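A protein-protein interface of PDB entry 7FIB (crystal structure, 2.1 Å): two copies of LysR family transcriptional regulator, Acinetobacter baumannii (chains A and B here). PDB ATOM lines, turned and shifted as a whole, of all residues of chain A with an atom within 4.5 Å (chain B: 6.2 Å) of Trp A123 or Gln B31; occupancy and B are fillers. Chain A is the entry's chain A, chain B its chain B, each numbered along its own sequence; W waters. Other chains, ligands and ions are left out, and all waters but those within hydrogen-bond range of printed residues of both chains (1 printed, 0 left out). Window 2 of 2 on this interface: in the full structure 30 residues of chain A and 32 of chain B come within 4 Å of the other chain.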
ATOM      1  N   ARG A 101      21.401  23.331  35.374  1.00  0.00           N
ATOM      2  CA  ARG A 101      20.299  23.538  34.440  1.00  0.00           C
ATOM      3  C   ARG A 101      19.216  24.430  35.049  1.00  0.00           C
ATOM      4  O   ARG A 101      18.717  24.153  36.136  1.00  0.00           O
ATOM      5  CB  ARG A 101      19.693  22.186  34.055  1.00  0.00           C
ATOM      6  CG  ARG A 101      19.126  22.112  32.656  1.00  0.00           C
ATOM      7  CD  ARG A 101      18.315  20.816  32.395  1.00  0.00           C
ATOM      8  NE  ARG A 101      18.984  19.550  32.751  1.00  0.00           N
ATOM      9  CZ  ARG A 101      19.911  18.945  32.025  1.00  0.00           C
ATOM     10  NH1 ARG A 101      20.326  19.489  30.886  1.00  0.00           N
ATOM     11  NH2 ARG A 101      20.427  17.787  32.435  1.00  0.00           N
ATOM     12  N   GLN A 102      18.817  25.471  34.320  1.00  0.00           N
ATOM     13  CA  GLN A 102      17.672  26.304  34.692  1.00  0.00           C
ATOM     14  C   GLN A 102      16.436  25.894  33.893  1.00  0.00           C
ATOM     15  O   GLN A 102      16.504  25.777  32.669  1.00  0.00           O
ATOM     16  CB  GLN A 102      17.977  27.786  34.454  1.00  0.00           C
ATOM     17  CG  GLN A 102      16.867  28.740  34.948  1.00  0.00           C
ATOM     18  CD  GLN A 102      17.167  30.205  34.652  1.00  0.00           C
ATOM     19  OE1 GLN A 102      18.306  30.582  34.374  1.00  0.00           O
ATOM     20  NE2 GLN A 102      16.140  31.043  34.733  1.00  0.00           N
ATOM     21  N   ILE A 103      15.308  25.685  34.571  1.00  0.00           N
ATOM     22  CA  ILE A 103      14.036  25.429  33.895  1.00  0.00           C
ATOM     23  C   ILE A 103      13.319  26.762  33.738  1.00  0.00           C
ATOM     24  O   ILE A 103      12.923  27.385  34.730  1.00  0.00           O
ATOM     25  CB  ILE A 103      13.160  24.424  34.665  1.00  0.00           C
ATOM     26  CG1 ILE A 103      13.968  23.199  35.149  1.00  0.00           C
ATOM     27  CG2 ILE A 103      11.926  24.040  33.851  1.00  0.00           C
ATOM     28  CD1 ILE A 103      14.721  22.394  34.071  1.00  0.00           C
ATOM     29  N   VAL A 104      13.152  27.205  32.503  1.00  0.00           N
ATOM     30  CA  VAL A 104      12.606  28.520  32.215  1.00  0.00           C
ATOM     31  C   VAL A 104      11.225  28.359  31.605  1.00  0.00           C
ATOM     32  O   VAL A 104      10.992  27.453  30.795  1.00  0.00           O
ATOM     33  CB  VAL A 104      13.531  29.312  31.274  1.00  0.00           C
ATOM     34  CG1 VAL A 104      12.990  30.713  31.072  1.00  0.00           C
ATOM     35  CG2 VAL A 104      14.927  29.380  31.859  1.00  0.00           C
ATOM     36  N   TYR A 122      19.775  25.693  29.842  1.00  0.00           N
ATOM     37  CA  TYR A 122      18.397  25.770  30.288  1.00  0.00           C
ATOM     38  C   TYR A 122      17.515  24.902  29.404  1.00  0.00           C
ATOM     39  O   TYR A 122      17.834  24.650  28.241  1.00  0.00           O
ATOM     40  CB  TYR A 122      17.903  27.212  30.275  1.00  0.00           C
ATOM     41  CG  TYR A 122      17.885  27.828  28.907  1.00  0.00           C
ATOM     42  CD1 TYR A 122      16.765  27.726  28.090  1.00  0.00           C
ATOM     43  CD2 TYR A 122      18.985  28.532  28.427  1.00  0.00           C
ATOM     44  CE1 TYR A 122      16.743  28.294  26.827  1.00  0.00           C
ATOM     45  CE2 TYR A 122      18.966  29.122  27.171  1.00  0.00           C
ATOM     46  CZ  TYR A 122      17.843  29.007  26.377  1.00  0.00           C
ATOM     47  OH  TYR A 122      17.818  29.584  25.120  1.00  0.00           O
ATOM     48  N   TRP A 123      16.393  24.459  29.976  1.00  0.00           N
ATOM     49  CA  TRP A 123      15.276  23.872  29.241  1.00  0.00           C
ATOM     50  C   TRP A 123      14.105  24.846  29.288  1.00  0.00           C
ATOM     51  O   TRP A 123      13.869  25.495  30.315  1.00  0.00           O
ATOM     52  CB  TRP A 123      14.820  22.559  29.852  1.00  0.00           C
ATOM     53  CG  TRP A 123      15.748  21.411  29.696  1.00  0.00           C
ATOM     54  CD1 TRP A 123      16.986  21.393  29.063  1.00  0.00           C
ATOM     55  CD2 TRP A 123      15.562  20.109  30.247  1.00  0.00           C
ATOM     56  NE1 TRP A 123      17.553  20.140  29.181  1.00  0.00           N
ATOM     57  CE2 TRP A 123      16.700  19.334  29.893  1.00  0.00           C
ATOM     58  CE3 TRP A 123      14.549  19.519  31.005  1.00  0.00           C
ATOM     59  CZ2 TRP A 123      16.834  18.014  30.265  1.00  0.00           C
ATOM     60  CZ3 TRP A 123      14.676  18.208  31.363  1.00  0.00           C
ATOM     61  CH2 TRP A 123      15.821  17.460  30.995  1.00  0.00           C
ATOM     62  N   ARG A 124      13.351  24.931  28.201  1.00  0.00           N
ATOM     63  CA  ARG A 124      12.191  25.801  28.150  1.00  0.00           C
ATOM     64  C   ARG A 124      10.911  24.980  28.168  1.00  0.00           C
ATOM     65  O   ARG A 124      10.796  23.952  27.489  1.00  0.00           O
ATOM     66  CB  ARG A 124      12.235  26.698  26.916  1.00  0.00           C
ATOM     67  CG  ARG A 124      11.039  27.578  26.735  1.00  0.00           C
ATOM     68  CD  ARG A 124      11.143  28.321  25.421  1.00  0.00           C
ATOM     69  NE  ARG A 124      10.997  27.399  24.302  1.00  0.00           N
ATOM     70  CZ  ARG A 124       9.830  26.932  23.862  1.00  0.00           C
ATOM     71  NH1 ARG A 124       8.682  27.311  24.437  1.00  0.00           N
ATOM     72  NH2 ARG A 124       9.813  26.091  22.841  1.00  0.00           N
ATOM     73  N   THR A 125       9.954  25.445  28.954  1.00  0.00           N
ATOM     74  CA  THR A 125       8.603  24.928  28.924  1.00  0.00           C
ATOM     75  C   THR A 125       7.668  26.125  28.944  1.00  0.00           C
ATOM     76  O   THR A 125       8.095  27.263  29.148  1.00  0.00           O
ATOM     77  CB  THR A 125       8.370  23.957  30.087  1.00  0.00           C
ATOM     78  OG1 THR A 125       7.053  23.417  30.007  1.00  0.00           O
ATOM     79  CG2 THR A 125       8.592  24.652  31.430  1.00  0.00           C
ATOM     80  N   MET A 134       9.381  19.201  36.818  1.00  0.00           N
ATOM     81  CA  MET A 134      10.738  18.816  36.468  1.00  0.00           C
ATOM     82  C   MET A 134      11.724  19.205  37.562  1.00  0.00           C
ATOM     83  O   MET A 134      12.614  18.416  37.908  1.00  0.00           O
ATOM     84  CB  MET A 134      11.104  19.425  35.116  1.00  0.00           C
ATOM     85  CG  MET A 134      10.273  18.826  33.970  1.00  0.00           C
ATOM     86  SD  MET A 134      10.987  19.096  32.344  1.00  0.00           S
ATOM     87  CE  MET A 134      10.029  20.515  31.742  1.00  0.00           C
ATOM     88  N   LEU A 139      15.723  17.864  37.991  1.00  0.00           N
ATOM     89  CA  LEU A 139      16.301  18.129  36.683  1.00  0.00           C
ATOM     90  C   LEU A 139      16.854  19.536  36.552  1.00  0.00           C
ATOM     91  O   LEU A 139      17.446  19.852  35.517  1.00  0.00           O
ATOM     92  CB  LEU A 139      15.255  17.886  35.598  1.00  0.00           C
ATOM     93  CG  LEU A 139      14.748  16.446  35.537  1.00  0.00           C
ATOM     94  CD1 LEU A 139      13.507  16.323  34.645  1.00  0.00           C
ATOM     95  CD2 LEU A 139      15.858  15.540  35.060  1.00  0.00           C
ATOM     96  N   PRO B   1      19.241  18.568  17.667  1.00  0.00           N
ATOM     97  CA  PRO B   1      20.145  19.088  18.707  1.00  0.00           C
ATOM     98  C   PRO B   1      19.363  19.419  19.980  1.00  0.00           C
ATOM     99  O   PRO B   1      19.903  19.554  21.088  1.00  0.00           O
ATOM    100  CB  PRO B   1      20.753  20.347  18.071  1.00  0.00           C
ATOM    101  CG  PRO B   1      19.945  20.603  16.799  1.00  0.00           C
ATOM    102  CD  PRO B   1      19.383  19.278  16.386  1.00  0.00           C
ATOM    103  N   ASN B   2      18.055  19.537  19.797  1.00  0.00           N
ATOM    104  CA  ASN B   2      17.117  19.708  20.887  1.00  0.00           C
ATOM    105  C   ASN B   2      15.941  18.792  20.609  1.00  0.00           C
ATOM    106  O   ASN B   2      15.738  18.342  19.482  1.00  0.00           O
ATOM    107  CB  ASN B   2      16.663  21.152  20.992  1.00  0.00           C
ATOM    108  CG  ASN B   2      16.085  21.637  19.702  1.00  0.00           C
ATOM    109  OD1 ASN B   2      15.482  20.866  18.947  1.00  0.00           O
ATOM    110  ND2 ASN B   2      16.314  22.912  19.397  1.00  0.00           N
ATOM    111  N   LEU B   3      15.171  18.506  21.649  1.00  0.00           N
ATOM    112  CA  LEU B   3      13.992  17.669  21.508  1.00  0.00           C
ATOM    113  C   LEU B   3      12.813  18.412  22.097  1.00  0.00           C
ATOM    114  O   LEU B   3      12.817  18.714  23.288  1.00  0.00           O
ATOM    115  CB  LEU B   3      14.187  16.317  22.203  1.00  0.00           C
ATOM    116  CG  LEU B   3      12.948  15.421  22.278  1.00  0.00           C
ATOM    117  CD1 LEU B   3      12.570  14.944  20.891  1.00  0.00           C
ATOM    118  CD2 LEU B   3      13.211  14.241  23.189  1.00  0.00           C
ATOM    119  N   THR B   4      11.806  18.690  21.271  1.00  0.00           N
ATOM    120  CA  THR B   4      10.547  19.274  21.720  1.00  0.00           C
ATOM    121  C   THR B   4       9.486  18.184  21.818  1.00  0.00           C
ATOM    122  O   THR B   4       9.166  17.530  20.821  1.00  0.00           O
ATOM    123  CB  THR B   4      10.070  20.361  20.756  1.00  0.00           C
ATOM    124  OG1 THR B   4      11.014  21.428  20.751  1.00  0.00           O
ATOM    125  CG2 THR B   4       8.718  20.900  21.207  1.00  0.00           C
ATOM    126  N   VAL B  20      10.931  11.994  30.502  1.00  0.00           N
ATOM    127  CA  VAL B  20      11.926  13.062  30.460  1.00  0.00           C
ATOM    128  C   VAL B  20      13.179  12.675  31.238  1.00  0.00           C
ATOM    129  O   VAL B  20      14.311  12.995  30.831  1.00  0.00           O
ATOM    130  CB  VAL B  20      11.303  14.368  31.002  1.00  0.00           C
ATOM    131  CG1 VAL B  20      12.349  15.461  31.122  1.00  0.00           C
ATOM    132  CG2 VAL B  20      10.142  14.810  30.119  1.00  0.00           C
ATOM    133  N   GLU B  24      16.992  12.390  29.791  1.00  0.00           N
ATOM    134  CA  GLU B  24      18.078  13.250  30.253  1.00  0.00           C
ATOM    135  C   GLU B  24      19.247  12.446  30.828  1.00  0.00           C
ATOM    136  O   GLU B  24      20.400  12.889  30.751  1.00  0.00           O
ATOM    137  CB  GLU B  24      17.545  14.277  31.269  1.00  0.00           C
ATOM    138  CG  GLU B  24      17.545  13.809  32.700  1.00  0.00           C
ATOM    139  CD  GLU B  24      18.880  14.021  33.417  1.00  0.00           C
ATOM    140  OE1 GLU B  24      19.678  14.911  33.019  1.00  0.00           O
ATOM    141  OE2 GLU B  24      19.110  13.290  34.390  1.00  0.00           O
ATOM    142  N   PHE B  27      21.013  11.356  27.580  1.00  0.00           N
ATOM    143  CA  PHE B  27      21.586  12.455  26.797  1.00  0.00           C
ATOM    144  C   PHE B  27      21.782  13.660  27.714  1.00  0.00           C
ATOM    145  O   PHE B  27      20.973  14.599  27.712  1.00  0.00           O
ATOM    146  CB  PHE B  27      20.717  12.791  25.583  1.00  0.00           C
ATOM    147  CG  PHE B  27      20.431  11.608  24.692  1.00  0.00           C
ATOM    148  CD1 PHE B  27      21.383  11.133  23.813  1.00  0.00           C
ATOM    149  CD2 PHE B  27      19.200  10.964  24.741  1.00  0.00           C
ATOM    150  CE1 PHE B  27      21.118  10.025  22.992  1.00  0.00           C
ATOM    151  CE2 PHE B  27      18.917   9.866  23.916  1.00  0.00           C
ATOM    152  CZ  PHE B  27      19.884   9.393  23.047  1.00  0.00           C
ATOM    153  N   ASP B  29      23.382  16.301  27.638  1.00  0.00           N
ATOM    154  CA  ASP B  29      23.518  17.618  27.035  1.00  0.00           C
ATOM    155  C   ASP B  29      22.322  17.998  26.175  1.00  0.00           C
ATOM    156  O   ASP B  29      22.336  19.057  25.541  1.00  0.00           O
ATOM    157  CB  ASP B  29      24.802  17.678  26.200  1.00  0.00           C
ATOM    158  CG  ASP B  29      26.053  17.784  27.062  1.00  0.00           C
ATOM    159  OD1 ASP B  29      25.942  18.284  28.209  1.00  0.00           O
ATOM    160  OD2 ASP B  29      27.137  17.349  26.600  1.00  0.00           O
ATOM    161  N   LEU B  30      21.296  17.160  26.117  1.00  0.00           N
ATOM    162  CA  LEU B  30      20.180  17.414  25.221  1.00  0.00           C
ATOM    163  C   LEU B  30      19.272  18.476  25.820  1.00  0.00           C
ATOM    164  O   LEU B  30      18.934  18.415  27.005  1.00  0.00           O
ATOM    165  CB  LEU B  30      19.397  16.129  24.977  1.00  0.00           C
ATOM    166  CG  LEU B  30      18.152  16.191  24.101  1.00  0.00           C
ATOM    167  CD1 LEU B  30      18.500  16.524  22.655  1.00  0.00           C
ATOM    168  CD2 LEU B  30      17.473  14.858  24.184  1.00  0.00           C
ATOM    169  N   GLN B  31      18.882  19.452  25.010  1.00  0.00           N
ATOM    170  CA  GLN B  31      17.873  20.397  25.460  1.00  0.00           C
ATOM    171  C   GLN B  31      16.494  19.808  25.205  1.00  0.00           C
ATOM    172  O   GLN B  31      16.111  19.569  24.052  1.00  0.00           O
ATOM    173  CB  GLN B  31      18.013  21.742  24.767  1.00  0.00           C
ATOM    174  CG  GLN B  31      17.136  22.794  25.425  1.00  0.00           C
ATOM    175  CD  GLN B  31      17.053  24.069  24.622  1.00  0.00           C
ATOM    176  OE1 GLN B  31      17.487  25.124  25.083  1.00  0.00           O
ATOM    177  NE2 GLN B  31      16.490  23.984  23.412  1.00  0.00           N
ATOM    178  N   ILE B  32      15.754  19.558  26.275  1.00  0.00           N
ATOM    179  CA  ILE B  32      14.415  18.980  26.183  1.00  0.00           C
ATOM    180  C   ILE B  32      13.416  20.077  26.500  1.00  0.00           C
ATOM    181  O   ILE B  32      13.433  20.625  27.604  1.00  0.00           O
ATOM    182  CB  ILE B  32      14.255  17.784  27.132  1.00  0.00           C
ATOM    183  CG1 ILE B  32      15.325  16.731  26.818  1.00  0.00           C
ATOM    184  CG2 ILE B  32      12.856  17.186  27.012  1.00  0.00           C
ATOM    185  CD1 ILE B  32      15.168  15.434  27.597  1.00  0.00           C
ATOM    186  N   ASN B  33      12.575  20.414  25.525  1.00  0.00           N
ATOM    187  CA  ASN B  33      11.531  21.422  25.662  1.00  0.00           C
ATOM    188  C   ASN B  33      10.166  20.742  25.756  1.00  0.00           C
ATOM    189  O   ASN B  33       9.731  20.085  24.809  1.00  0.00           O
ATOM    190  CB  ASN B  33      11.572  22.392  24.487  1.00  0.00           C
ATOM    191  CG  ASN B  33      12.875  23.176  24.441  1.00  0.00           C
ATOM    192  OD1 ASN B  33      13.395  23.606  25.484  1.00  0.00           O
ATOM    193  ND2 ASN B  33      13.446  23.306  23.241  1.00  0.00           N
ATOM    194  N   ILE B  34       9.510  20.887  26.900  1.00  0.00           N
ATOM    195  CA  ILE B  34       8.191  20.319  27.159  1.00  0.00           C
ATOM    196  C   ILE B  34       7.180  21.420  26.911  1.00  0.00           C
ATOM    197  O   ILE B  34       7.099  22.372  27.686  1.00  0.00           O
ATOM    198  CB  ILE B  34       8.070  19.788  28.594  1.00  0.00           C
ATOM    199  CG1 ILE B  34       9.227  18.851  28.928  1.00  0.00           C
ATOM    200  CG2 ILE B  34       6.705  19.094  28.816  1.00  0.00           C
ATOM    201  CD1 ILE B  34       9.388  17.686  27.946  1.00  0.00           C
HETATM  202  O   HOH W   1       4.257  21.787  29.146  1.00  0.00           O
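No position is printed for both chains.
Water W1 lies within hydrogen-bond range of O of Ile B34 (3.2 Å) and OG1 of Thr A125 (3.3 Å).
Gln B31 touches just these residues of chain A: Tyr A122 and Trp A123. Printed residues of chain B within 4 Å of Leu A139: Val B20 and Glu B24. Printed residues of chain A within 4 Å of Ile B32: Trp A123. Of the printed residues of chain A, Asn B33 touches Arg A124 (3.0 Å). Val A104 touches none of the printed residues of chain B. Pro B1 touches none of the printed residues of chain A. The nearest residue of chain B that does not touch Trp A123 is Asn B33 (4.1 Å). The nearest printed residue of chain A that does not touch Gln B31 is Arg A124 (5.2 Å).
The backbone NH (N) of Leu B3 lies within hydrogen-bond range of the backbone carbonyl oxygen (O) of Gln B31 (2.8 Å). N of Trp A123 sits at hydrogen-bond distance from O of Gln A102 (3.0 Å). The backbone carbonyl oxygen of Leu B3 lies within hydrogen-bond range of the backbone NH of Asn B33 (2.8 Å). The backbone carbonyl oxygen of Val A104 is in hydrogen-bond range of the backbone NH of Thr A125. The backbone NH (N) of Val A104 is in hydrogen-bond range of the backbone carbonyl oxygen (O) of Trp A123. NE of Arg A101 lies within hydrogen-bond range of O of Leu A139, 3.2 Å away.
Along chain B the printed residues that touch a printed residue of chain A span positions 20 to 34. Of the 10 printed residues of chain A, 7 touch a printed residue of chain B. Printed residues of chain A that touch a printed residue of chain B: Arg A101, Tyr A122, Trp A123, Arg A124, Thr A125, Met A134 and Leu A139.
Among the printed residues, merely in contact across the chains: Trp A123 with Val B20 (3.6 Å), Trp A123 with Glu B24 (3.6 Å), Trp A123 with Gln B31 (3.7 Å), Met A134 with Ile B34 (3.4 Å), Leu A139 with Val B20 (3.8 Å) and Leu A139 with Glu B24 (3.4 Å).
The backbone NH (N) of Ile B34 is in hydrogen-bond range of the backbone carbonyl oxygen (O) of Arg A124 (3.4 Å). The guanidinium group (NH2) of Arg A101 is in salt-bridge range of the side-chain carboxylate (OE1) of Glu B24 (3.0 Å). The backbone carbonyl oxygen of Leu B30 is in hydrogen-bond range of the indole nitrogen of Trp A123 (3.1 Å). O of Tyr A122 sits close to OE1 of Gln B31. OG1 of Thr A125 lies within hydrogen-bond range of O of Ile B34 (2.5 Å). The side-chain amide oxygen (OD1) of Asn B33 is in hydrogen-bond range of the backbone NH (N) of Arg A124, 3.0 Å away. The indole nitrogen (NE1) of Trp A123 sits close to the backbone NH (N) of Ile B32.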
